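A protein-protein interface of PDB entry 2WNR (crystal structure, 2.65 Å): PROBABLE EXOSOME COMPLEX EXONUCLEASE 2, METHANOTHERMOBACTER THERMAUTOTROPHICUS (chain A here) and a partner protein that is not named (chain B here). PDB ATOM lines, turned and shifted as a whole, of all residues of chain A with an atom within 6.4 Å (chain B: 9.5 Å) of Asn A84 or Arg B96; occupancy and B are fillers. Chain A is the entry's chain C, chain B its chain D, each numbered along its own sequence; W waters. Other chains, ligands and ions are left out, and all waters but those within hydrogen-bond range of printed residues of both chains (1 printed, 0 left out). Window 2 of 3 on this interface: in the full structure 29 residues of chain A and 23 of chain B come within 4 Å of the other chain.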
ATOM      1  N   LEU A  82      11.453   2.473  -1.530  1.00  0.00           N
ATOM      2  CA  LEU A  82      12.179   2.317  -0.273  1.00  0.00           C
ATOM      3  C   LEU A  82      13.244   1.222  -0.377  1.00  0.00           C
ATOM      4  O   LEU A  82      12.925   0.039  -0.429  1.00  0.00           O
ATOM      5  CB  LEU A  82      11.192   2.017   0.864  1.00  0.00           C
ATOM      6  CG  LEU A  82      10.310   3.196   1.306  1.00  0.00           C
ATOM      7  CD1 LEU A  82       8.995   2.731   1.909  1.00  0.00           C
ATOM      8  CD2 LEU A  82      11.049   4.099   2.288  1.00  0.00           C
ATOM      9  N   THR A  83      14.511   1.623  -0.408  1.00  0.00           N
ATOM     10  CA  THR A  83      15.609   0.677  -0.531  1.00  0.00           C
ATOM     11  C   THR A  83      16.220   0.410   0.839  1.00  0.00           C
ATOM     12  O   THR A  83      16.584   1.343   1.567  1.00  0.00           O
ATOM     13  CB  THR A  83      16.718   1.205  -1.488  1.00  0.00           C
ATOM     14  OG1 THR A  83      16.159   1.554  -2.750  1.00  0.00           O
ATOM     15  CG2 THR A  83      17.810   0.168  -1.719  1.00  0.00           C
ATOM     16  N   ASN A  84      16.337  -0.869   1.180  1.00  0.00           N
ATOM     17  CA  ASN A  84      17.014  -1.292   2.396  1.00  0.00           C
ATOM     18  C   ASN A  84      17.849  -2.548   2.132  1.00  0.00           C
ATOM     19  O   ASN A  84      17.482  -3.397   1.311  1.00  0.00           O
ATOM     20  CB  ASN A  84      16.013  -1.529   3.538  1.00  0.00           C
ATOM     21  CG  ASN A  84      16.696  -1.977   4.818  1.00  0.00           C
ATOM     22  OD1 ASN A  84      17.370  -1.180   5.483  1.00  0.00           O
ATOM     23  ND2 ASN A  84      16.564  -3.268   5.151  1.00  0.00           N
ATOM     24  N   SER A  85      18.970  -2.674   2.819  1.00  0.00           N
ATOM     25  CA  SER A  85      19.812  -3.841   2.622  1.00  0.00           C
ATOM     26  C   SER A  85      20.184  -4.480   3.946  1.00  0.00           C
ATOM     27  O   SER A  85      20.428  -3.785   4.926  1.00  0.00           O
ATOM     28  CB  SER A  85      21.070  -3.470   1.847  1.00  0.00           C
ATOM     29  OG  SER A  85      21.716  -2.395   2.486  1.00  0.00           O
ATOM     30  N   GLU A  86      20.201  -5.808   3.958  1.00  0.00           N
ATOM     31  CA  GLU A  86      20.601  -6.564   5.119  1.00  0.00           C
ATOM     32  C   GLU A  86      21.960  -7.213   4.870  1.00  0.00           C
ATOM     33  O   GLU A  86      22.066  -8.196   4.143  1.00  0.00           O
ATOM     34  CB  GLU A  86      19.554  -7.611   5.444  1.00  0.00           C
ATOM     35  CG  GLU A  86      18.316  -7.043   6.005  1.00  0.00           C
ATOM     36  CD  GLU A  86      18.457  -6.585   7.427  1.00  0.00           C
ATOM     37  OE1 GLU A  86      18.613  -7.441   8.323  1.00  0.00           O
ATOM     38  OE2 GLU A  86      18.367  -5.365   7.649  1.00  0.00           O
ATOM     39  N   PRO A 100      21.006  -1.885  10.465  1.00  0.00           N
ATOM     40  CA  PRO A 100      22.039  -1.555   9.466  1.00  0.00           C
ATOM     41  C   PRO A 100      23.141  -0.601   9.954  1.00  0.00           C
ATOM     42  O   PRO A 100      22.854   0.512  10.409  1.00  0.00           O
ATOM     43  CB  PRO A 100      21.238  -0.918   8.331  1.00  0.00           C
ATOM     44  CG  PRO A 100      19.838  -1.476   8.488  1.00  0.00           C
ATOM     45  CD  PRO A 100      19.638  -1.608   9.966  1.00  0.00           C
ATOM     46  N   SER A 104      26.262  -0.933   5.610  1.00  0.00           N
ATOM     47  CA  SER A 104      24.970  -1.293   5.027  1.00  0.00           C
ATOM     48  C   SER A 104      24.268  -0.065   4.467  1.00  0.00           C
ATOM     49  O   SER A 104      23.850  -0.050   3.314  1.00  0.00           O
ATOM     50  CB  SER A 104      24.083  -1.958   6.069  1.00  0.00           C
ATOM     51  OG  SER A 104      22.912  -2.492   5.488  1.00  0.00           O
ATOM     52  N   VAL A 105      24.151   0.962   5.298  1.00  0.00           N
ATOM     53  CA  VAL A 105      23.508   2.216   4.934  1.00  0.00           C
ATOM     54  C   VAL A 105      24.087   2.812   3.649  1.00  0.00           C
ATOM     55  O   VAL A 105      23.330   3.284   2.784  1.00  0.00           O
ATOM     56  CB  VAL A 105      23.616   3.247   6.082  1.00  0.00           C
ATOM     57  CG1 VAL A 105      23.255   4.624   5.591  1.00  0.00           C
ATOM     58  CG2 VAL A 105      22.720   2.858   7.242  1.00  0.00           C
ATOM     59  N   GLU A 106      25.415   2.800   3.518  1.00  0.00           N
ATOM     60  CA  GLU A 106      26.035   3.370   2.339  1.00  0.00           C
ATOM     61  C   GLU A 106      25.640   2.553   1.121  1.00  0.00           C
ATOM     62  O   GLU A 106      25.136   3.090   0.138  1.00  0.00           O
ATOM     63  CB  GLU A 106      27.552   3.428   2.470  1.00  0.00           C
ATOM     64  CG  GLU A 106      28.214   4.075   1.271  1.00  0.00           C
ATOM     65  CD  GLU A 106      29.685   3.763   1.179  1.00  0.00           C
ATOM     66  OE1 GLU A 106      30.111   2.752   1.783  1.00  0.00           O
ATOM     67  OE2 GLU A 106      30.421   4.519   0.497  1.00  0.00           O
ATOM     68  N   SER A 108      23.190   0.650   0.665  1.00  0.00           N
ATOM     69  CA  SER A 108      21.766   0.837   0.436  1.00  0.00           C
ATOM     70  C   SER A 108      21.448   2.146  -0.272  1.00  0.00           C
ATOM     71  O   SER A 108      20.762   2.145  -1.290  1.00  0.00           O
ATOM     72  CB  SER A 108      21.026   0.770   1.757  1.00  0.00           C
ATOM     73  OG  SER A 108      19.684   0.406   1.543  1.00  0.00           O
ATOM     74  N   ARG A 109      21.968   3.252   0.255  1.00  0.00           N
ATOM     75  CA  ARG A 109      21.789   4.572  -0.346  1.00  0.00           C
ATOM     76  C   ARG A 109      22.388   4.736  -1.730  1.00  0.00           C
ATOM     77  O   ARG A 109      21.811   5.437  -2.569  1.00  0.00           O
ATOM     78  CB  ARG A 109      22.367   5.639   0.564  1.00  0.00           C
ATOM     79  CG  ARG A 109      21.509   5.869   1.779  1.00  0.00           C
ATOM     80  CD  ARG A 109      22.123   6.865   2.703  1.00  0.00           C
ATOM     81  NE  ARG A 109      22.188   8.195   2.109  1.00  0.00           N
ATOM     82  CZ  ARG A 109      21.174   9.058   2.057  1.00  0.00           C
ATOM     83  NH1 ARG A 109      19.985   8.742   2.541  1.00  0.00           N
ATOM     84  NH2 ARG A 109      21.357  10.244   1.509  1.00  0.00           N
ATOM     85  N   ASP A 112      20.064   2.932  -4.028  1.00  0.00           N
ATOM     86  CA  ASP A 112      18.859   3.742  -4.154  1.00  0.00           C
ATOM     87  C   ASP A 112      19.121   4.906  -5.095  1.00  0.00           C
ATOM     88  O   ASP A 112      18.272   5.253  -5.911  1.00  0.00           O
ATOM     89  CB  ASP A 112      18.397   4.238  -2.780  1.00  0.00           C
ATOM     90  CG  ASP A 112      17.086   5.012  -2.837  1.00  0.00           C
ATOM     91  OD1 ASP A 112      17.112   6.226  -3.140  1.00  0.00           O
ATOM     92  OD2 ASP A 112      16.030   4.405  -2.558  1.00  0.00           O
ATOM     93  N   PHE A 138       8.939  -1.622  -1.861  1.00  0.00           N
ATOM     94  CA  PHE A 138      10.027  -1.997  -0.949  1.00  0.00           C
ATOM     95  C   PHE A 138      11.077  -2.836  -1.677  1.00  0.00           C
ATOM     96  O   PHE A 138      10.855  -4.007  -1.976  1.00  0.00           O
ATOM     97  CB  PHE A 138       9.490  -2.759   0.259  1.00  0.00           C
ATOM     98  CG  PHE A 138       8.742  -1.906   1.222  1.00  0.00           C
ATOM     99  CD1 PHE A 138       9.401  -1.285   2.281  1.00  0.00           C
ATOM    100  CD2 PHE A 138       7.369  -1.712   1.076  1.00  0.00           C
ATOM    101  CE1 PHE A 138       8.699  -0.485   3.189  1.00  0.00           C
ATOM    102  CE2 PHE A 138       6.665  -0.916   1.966  1.00  0.00           C
ATOM    103  CZ  PHE A 138       7.331  -0.302   3.030  1.00  0.00           C
ATOM    104  N   LEU A 139      12.198  -2.215  -2.000  1.00  0.00           N
ATOM    105  CA  LEU A 139      13.340  -2.947  -2.523  1.00  0.00           C
ATOM    106  C   LEU A 139      14.158  -3.441  -1.341  1.00  0.00           C
ATOM    107  O   LEU A 139      14.722  -2.635  -0.592  1.00  0.00           O
ATOM    108  CB  LEU A 139      14.188  -2.046  -3.420  1.00  0.00           C
ATOM    109  CG  LEU A 139      13.708  -1.725  -4.844  1.00  0.00           C
ATOM    110  CD1 LEU A 139      12.207  -1.637  -4.995  1.00  0.00           C
ATOM    111  CD2 LEU A 139      14.368  -0.451  -5.307  1.00  0.00           C
ATOM    112  N   ASP A 140      14.192  -4.760  -1.156  1.00  0.00           N
ATOM    113  CA  ASP A 140      14.956  -5.356  -0.062  1.00  0.00           C
ATOM    114  C   ASP A 140      16.166  -6.173  -0.552  1.00  0.00           C
ATOM    115  O   ASP A 140      16.010  -7.172  -1.260  1.00  0.00           O
ATOM    116  CB  ASP A 140      14.018  -6.181   0.812  1.00  0.00           C
ATOM    117  CG  ASP A 140      13.196  -5.313   1.739  1.00  0.00           C
ATOM    118  OD1 ASP A 140      13.835  -4.576   2.541  1.00  0.00           O
ATOM    119  OD2 ASP A 140      11.930  -5.364   1.657  1.00  0.00           O
ATOM    120  N   LEU A 141      17.367  -5.731  -0.194  1.00  0.00           N
ATOM    121  CA  LEU A 141      18.608  -6.391  -0.655  1.00  0.00           C
ATOM    122  C   LEU A 141      19.134  -7.305   0.421  1.00  0.00           C
ATOM    123  O   LEU A 141      19.359  -6.867   1.544  1.00  0.00           O
ATOM    124  CB  LEU A 141      19.672  -5.368  -1.040  1.00  0.00           C
ATOM    125  CG  LEU A 141      19.475  -4.529  -2.304  1.00  0.00           C
ATOM    126  CD1 LEU A 141      18.075  -3.920  -2.390  1.00  0.00           C
ATOM    127  CD2 LEU A 141      20.513  -3.435  -2.375  1.00  0.00           C
ATOM    128  N   HIS A 142      19.312  -8.578   0.085  1.00  0.00           N
ATOM    129  CA  HIS A 142      19.646  -9.586   1.086  1.00  0.00           C
ATOM    130  C   HIS A 142      21.015 -10.157   0.751  1.00  0.00           C
ATOM    131  O   HIS A 142      21.148 -11.012  -0.140  1.00  0.00           O
ATOM    132  CB  HIS A 142      18.579 -10.687   1.112  1.00  0.00           C
ATOM    133  CG  HIS A 142      18.180 -11.117   2.487  1.00  0.00           C
ATOM    134  ND1 HIS A 142      17.604 -10.260   3.396  1.00  0.00           N
ATOM    135  CD2 HIS A 142      18.245 -12.324   3.099  1.00  0.00           C
ATOM    136  CE1 HIS A 142      17.338 -10.917   4.513  1.00  0.00           C
ATOM    137  NE2 HIS A 142      17.720 -12.171   4.360  1.00  0.00           N
ATOM    138  N   TYR B  79      28.447  13.623  12.049  1.00  0.00           N
ATOM    139  CA  TYR B  79      27.745  14.755  11.443  1.00  0.00           C
ATOM    140  C   TYR B  79      26.332  14.717  11.990  1.00  0.00           C
ATOM    141  O   TYR B  79      25.642  13.708  11.863  1.00  0.00           O
ATOM    142  CB  TYR B  79      27.746  14.618   9.912  1.00  0.00           C
ATOM    143  CG  TYR B  79      26.742  15.476   9.154  1.00  0.00           C
ATOM    144  CD1 TYR B  79      27.153  16.601   8.430  1.00  0.00           C
ATOM    145  CD2 TYR B  79      25.388  15.144   9.136  1.00  0.00           C
ATOM    146  CE1 TYR B  79      26.236  17.384   7.721  1.00  0.00           C
ATOM    147  CE2 TYR B  79      24.454  15.919   8.441  1.00  0.00           C
ATOM    148  CZ  TYR B  79      24.879  17.033   7.732  1.00  0.00           C
ATOM    149  OH  TYR B  79      23.934  17.776   7.049  1.00  0.00           O
ATOM    150  N   LYS B  90      13.394  18.486  12.612  1.00  0.00           N
ATOM    151  CA  LYS B  90      13.969  17.157  12.444  1.00  0.00           C
ATOM    152  C   LYS B  90      14.145  16.488  13.810  1.00  0.00           C
ATOM    153  O   LYS B  90      14.979  16.922  14.605  1.00  0.00           O
ATOM    154  CB  LYS B  90      15.324  17.245  11.717  1.00  0.00           C
ATOM    155  CG  LYS B  90      15.917  15.891  11.374  1.00  0.00           C
ATOM    156  CD  LYS B  90      17.029  15.985  10.329  1.00  0.00           C
ATOM    157  CE  LYS B  90      17.821  14.665  10.233  1.00  0.00           C
ATOM    158  NZ  LYS B  90      18.512  14.308  11.534  1.00  0.00           N
ATOM    159  N   GLY B  93      18.476  12.659  16.774  1.00  0.00           N
ATOM    160  CA  GLY B  93      18.848  11.267  16.612  1.00  0.00           C
ATOM    161  C   GLY B  93      19.400  11.038  15.214  1.00  0.00           C
ATOM    162  O   GLY B  93      19.222  11.882  14.313  1.00  0.00           O
ATOM    163  N   PRO B  94      20.050   9.882  15.008  1.00  0.00           N
ATOM    164  CA  PRO B  94      20.762   9.718  13.755  1.00  0.00           C
ATOM    165  C   PRO B  94      19.796   9.174  12.674  1.00  0.00           C
ATOM    166  O   PRO B  94      18.865   8.393  12.977  1.00  0.00           O
ATOM    167  CB  PRO B  94      21.862   8.706  14.126  1.00  0.00           C
ATOM    168  CG  PRO B  94      21.197   7.845  15.275  1.00  0.00           C
ATOM    169  CD  PRO B  94      19.935   8.600  15.733  1.00  0.00           C
ATOM    170  N   ASP B  95      19.995   9.624  11.437  1.00  0.00           N
ATOM    171  CA  ASP B  95      19.239   9.103  10.315  1.00  0.00           C
ATOM    172  C   ASP B  95      20.213   8.591   9.271  1.00  0.00           C
ATOM    173  O   ASP B  95      21.425   8.775   9.401  1.00  0.00           O
ATOM    174  CB  ASP B  95      18.265  10.153   9.749  1.00  0.00           C
ATOM    175  CG  ASP B  95      18.971  11.333   9.075  1.00  0.00           C
ATOM    176  OD1 ASP B  95      18.365  11.906   8.140  1.00  0.00           O
ATOM    177  OD2 ASP B  95      20.108  11.695   9.467  1.00  0.00           O
ATOM    178  N   ARG B  96      19.680   7.945   8.244  1.00  0.00           N
ATOM    179  CA  ARG B  96      20.501   7.265   7.262  1.00  0.00           C
ATOM    180  C   ARG B  96      21.459   8.207   6.536  1.00  0.00           C
ATOM    181  O   ARG B  96      22.622   7.866   6.315  1.00  0.00           O
ATOM    182  CB  ARG B  96      19.611   6.510   6.287  1.00  0.00           C
ATOM    183  CG  ARG B  96      19.021   5.255   6.889  1.00  0.00           C
ATOM    184  CD  ARG B  96      17.907   4.711   6.047  1.00  0.00           C
ATOM    185  NE  ARG B  96      18.332   4.254   4.724  1.00  0.00           N
ATOM    186  CZ  ARG B  96      18.716   3.011   4.447  1.00  0.00           C
ATOM    187  NH1 ARG B  96      18.757   2.085   5.406  1.00  0.00           N
ATOM    188  NH2 ARG B  96      19.053   2.696   3.204  1.00  0.00           N
ATOM    189  N   ARG B  97      20.966   9.396   6.197  1.00  0.00           N
ATOM    190  CA  ARG B  97      21.757  10.407   5.518  1.00  0.00           C
ATOM    191  C   ARG B  97      22.902  10.891   6.409  1.00  0.00           C
ATOM    192  O   ARG B  97      24.041  11.022   5.941  1.00  0.00           O
ATOM    193  CB  ARG B  97      20.866  11.573   5.089  1.00  0.00           C
ATOM    194  CG  ARG B  97      21.584  12.715   4.404  1.00  0.00           C
ATOM    195  CD  ARG B  97      20.671  13.917   4.233  1.00  0.00           C
ATOM    196  NE  ARG B  97      21.431  15.135   3.971  1.00  0.00           N
ATOM    197  CZ  ARG B  97      21.851  15.980   4.911  1.00  0.00           C
ATOM    198  NH1 ARG B  97      21.579  15.748   6.193  1.00  0.00           N
ATOM    199  NH2 ARG B  97      22.542  17.062   4.574  1.00  0.00           N
ATOM    200  N   SER B  98      22.608  11.154   7.685  1.00  0.00           N
ATOM    201  CA  SER B  98      23.646  11.558   8.645  1.00  0.00           C
ATOM    202  C   SER B  98      24.711  10.499   8.823  1.00  0.00           C
ATOM    203  O   SER B  98      25.870  10.817   8.968  1.00  0.00           O
ATOM    204  CB  SER B  98      23.046  11.870  10.012  1.00  0.00           C
ATOM    205  OG  SER B  98      22.420  13.141   9.996  1.00  0.00           O
ATOM    206  N   VAL B  99      24.304   9.236   8.829  1.00  0.00           N
ATOM    207  CA  VAL B  99      25.218   8.119   8.990  1.00  0.00           C
ATOM    208  C   VAL B  99      26.148   8.006   7.799  1.00  0.00           C
ATOM    209  O   VAL B  99      27.330   7.700   7.973  1.00  0.00           O
ATOM    210  CB  VAL B  99      24.454   6.780   9.197  1.00  0.00           C
ATOM    211  CG1 VAL B  99      25.344   5.581   8.875  1.00  0.00           C
ATOM    212  CG2 VAL B  99      23.922   6.681  10.628  1.00  0.00           C
ATOM    213  N   GLU B 100      25.626   8.248   6.592  1.00  0.00           N
ATOM    214  CA  GLU B 100      26.458   8.176   5.383  1.00  0.00           C
ATOM    215  C   GLU B 100      27.460   9.311   5.358  1.00  0.00           C
ATOM    216  O   GLU B 100      28.627   9.098   5.052  1.00  0.00           O
ATOM    217  CB  GLU B 100      25.621   8.201   4.103  1.00  0.00           C
ATOM    218  CG  GLU B 100      26.449   7.878   2.857  1.00  0.00           C
ATOM    219  CD  GLU B 100      25.804   8.315   1.541  1.00  0.00           C
ATOM    220  OE1 GLU B 100      24.614   8.709   1.539  1.00  0.00           O
ATOM    221  OE2 GLU B 100      26.497   8.258   0.498  1.00  0.00           O
ATOM    222  N   ILE B 101      27.009  10.519   5.684  1.00  0.00           N
ATOM    223  CA  ILE B 101      27.878  11.687   5.646  1.00  0.00           C
ATOM    224  C   ILE B 101      29.011  11.527   6.653  1.00  0.00           C
ATOM    225  O   ILE B 101      30.172  11.837   6.344  1.00  0.00           O
ATOM    226  CB  ILE B 101      27.117  13.000   5.889  1.00  0.00           C
ATOM    227  CG1 ILE B 101      26.094  13.238   4.766  1.00  0.00           C
ATOM    228  CG2 ILE B 101      28.098  14.171   5.983  1.00  0.00           C
ATOM    229  CD1 ILE B 101      25.169  14.427   4.996  1.00  0.00           C
ATOM    230  N   SER B 102      28.678  11.021   7.838  1.00  0.00           N
ATOM    231  CA  SER B 102      29.669  10.765   8.871  1.00  0.00           C
ATOM    232  C   SER B 102      30.722   9.786   8.373  1.00  0.00           C
ATOM    233  O   SER B 102      31.931   9.984   8.605  1.00  0.00           O
ATOM    234  CB  SER B 102      29.015  10.233  10.144  1.00  0.00           C
ATOM    235  OG  SER B 102      28.002  11.112  10.618  1.00  0.00           O
ATOM    236  N   LYS B 103      30.266   8.751   7.664  1.00  0.00           N
ATOM    237  CA  LYS B 103      31.160   7.730   7.111  1.00  0.00           C
ATOM    238  C   LYS B 103      32.171   8.320   6.122  1.00  0.00           C
ATOM    239  O   LYS B 103      33.379   8.125   6.269  1.00  0.00           O
ATOM    240  CB  LYS B 103      30.354   6.610   6.455  1.00  0.00           C
ATOM    241  CG  LYS B 103      31.154   5.369   6.128  1.00  0.00           C
ATOM    242  CD  LYS B 103      30.413   4.504   5.125  1.00  0.00           C
ATOM    243  CE  LYS B 103      30.957   3.088   5.087  1.00  0.00           C
ATOM    244  NZ  LYS B 103      32.374   3.050   4.728  1.00  0.00           N
ATOM    245  N   ILE B 104      31.674   9.057   5.133  1.00  0.00           N
ATOM    246  CA  ILE B 104      32.546   9.586   4.075  1.00  0.00           C
ATOM    247  C   ILE B 104      33.382  10.806   4.498  1.00  0.00           C
ATOM    248  O   ILE B 104      34.412  11.093   3.878  1.00  0.00           O
ATOM    249  CB  ILE B 104      31.778   9.858   2.744  1.00  0.00           C
ATOM    250  CG1 ILE B 104      30.756  10.976   2.915  1.00  0.00           C
ATOM    251  CG2 ILE B 104      31.129   8.582   2.237  1.00  0.00           C
ATOM    252  CD1 ILE B 104      29.937  11.262   1.665  1.00  0.00           C
ATOM    253  N   ARG B 137      27.592  18.907   3.760  1.00  0.00           N
ATOM    254  CA  ARG B 137      28.612  17.873   3.920  1.00  0.00           C
ATOM    255  C   ARG B 137      29.992  18.419   3.550  1.00  0.00           C
ATOM    256  O   ARG B 137      30.976  18.131   4.226  1.00  0.00           O
ATOM    257  CB  ARG B 137      28.260  16.591   3.150  1.00  0.00           C
ATOM    258  CG  ARG B 137      28.443  16.661   1.643  1.00  0.00           C
ATOM    259  CD  ARG B 137      27.802  15.493   0.962  1.00  0.00           C
ATOM    260  NE  ARG B 137      26.364  15.506   1.172  1.00  0.00           N
ATOM    261  CZ  ARG B 137      25.593  14.430   1.063  1.00  0.00           C
ATOM    262  NH1 ARG B 137      26.134  13.254   0.744  1.00  0.00           N
ATOM    263  NH2 ARG B 137      24.282  14.526   1.281  1.00  0.00           N
ATOM    264  N   GLN B 202      31.101  12.569  -4.888  1.00  0.00           N
ATOM    265  CA  GLN B 202      29.795  11.965  -5.155  1.00  0.00           C
ATOM    266  C   GLN B 202      29.158  12.632  -6.365  1.00  0.00           C
ATOM    267  O   GLN B 202      29.620  13.674  -6.823  1.00  0.00           O
ATOM    268  CB  GLN B 202      28.857  12.092  -3.955  1.00  0.00           C
ATOM    269  CG  GLN B 202      29.320  11.394  -2.705  1.00  0.00           C
ATOM    270  CD  GLN B 202      28.351  11.592  -1.559  1.00  0.00           C
ATOM    271  OE1 GLN B 202      28.158  12.709  -1.081  1.00  0.00           O
ATOM    272  NE2 GLN B 202      27.716  10.506  -1.123  1.00  0.00           N
HETATM  273  O   HOH W   1      24.199  11.310   0.051  1.00  0.00           O
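Among the printed residues, pairs that only touch across the chains: Asn A84 with Arg B96, Val A105 with Arg B96, Arg A109 with Arg B96 and Arg A109 with Arg B97.
Water W1 lies within hydrogen-bond range of NH1 of Arg B137 (2.8 Å), OE1 of Glu B100 (3.0 Å) and NH2 of Arg A109 (3.4 Å).
O of Leu A139 sits at hydrogen-bond distance from N of Asn A84 (3.0 Å).
The side-chain hydroxyl of Ser A108 is in hydrogen-bond range of the backbone NH of Ser A85, at 3.4 Å.
OG1 of Thr A83 lies within hydrogen-bond range of OD2 of Asp A112, 2.9 Å away.
NE2 of Gln B202 is in hydrogen-bond range of OE2 of Glu B100, 3.0 Å away.
The backbone carbonyl oxygen (O) of Thr A83 sits at hydrogen-bond distance from the side-chain hydroxyl (OG) of Ser A108.
The side-chain hydroxyl of Tyr B79 is in hydrogen-bond range of the guanidinium group of Arg B97 (2.9 Å).
Hydrophobic or aromatic side chains of chain A within 4 Å of the printed part of chain B: Val A105.
Of the 16 printed residues of chain B, 4 touch a printed residue of chain A.
Printed residues of chain B that touch a printed residue of chain A: Arg B96, Arg B97, Glu B100 and Lys B103.
Along chain B the printed residues that touch a printed residue of chain A span positions 96 to 103.
Among the printed residues, 8 pairs touch across the chains.
Thr A83 touches one residue of chain B.
Asn A84 touches just one residue of chain B: Arg B96.
No residue of chain B comes within 4 Å of Ser A85.
Of the printed residues of chain B, Glu A106 touches Lys B103 (3.4 Å).
Phe A138 touches none of the printed residues of chain B.
No residue of chain B comes within 4 Å of Leu A141.
Of the printed residues of chain A, Arg B96 touches Thr A83 (3.3 Å), Asn A84 (3.5 Å), Val A105 (3.4 Å), Ser A108 (2.9 Å) and Arg A109 (3.8 Å).
Of the printed residues of chain A, Arg B97 touches Arg A109 (3.8 Å).
Of the printed residues of chain A, Glu B100 touches Arg A109 (2.5 Å).
Printed residues of chain A within 4 Å of Lys B103: Glu A106.
The nearest printed residue of chain B that does not touch Asn A84 is Asp B95 (10.9 Å).
The nearest residue of chain A that does not touch Arg B96 is Pro A100 (4.8 Å).
O of Thr A83 is in hydrogen-bond range of NH2 of Arg B96.
NZ of Lys B103 is in salt-bridge range of OE1 of Glu A106, 3.7 Å away.
The guanidinium group (NH2) of Arg B96 is in hydrogen-bond range of the side-chain hydroxyl (OG) of Ser A108 (2.9 Å).
NE of Arg A109 lies within salt-bridge range of OE1 of Glu B100 (2.5 Å).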
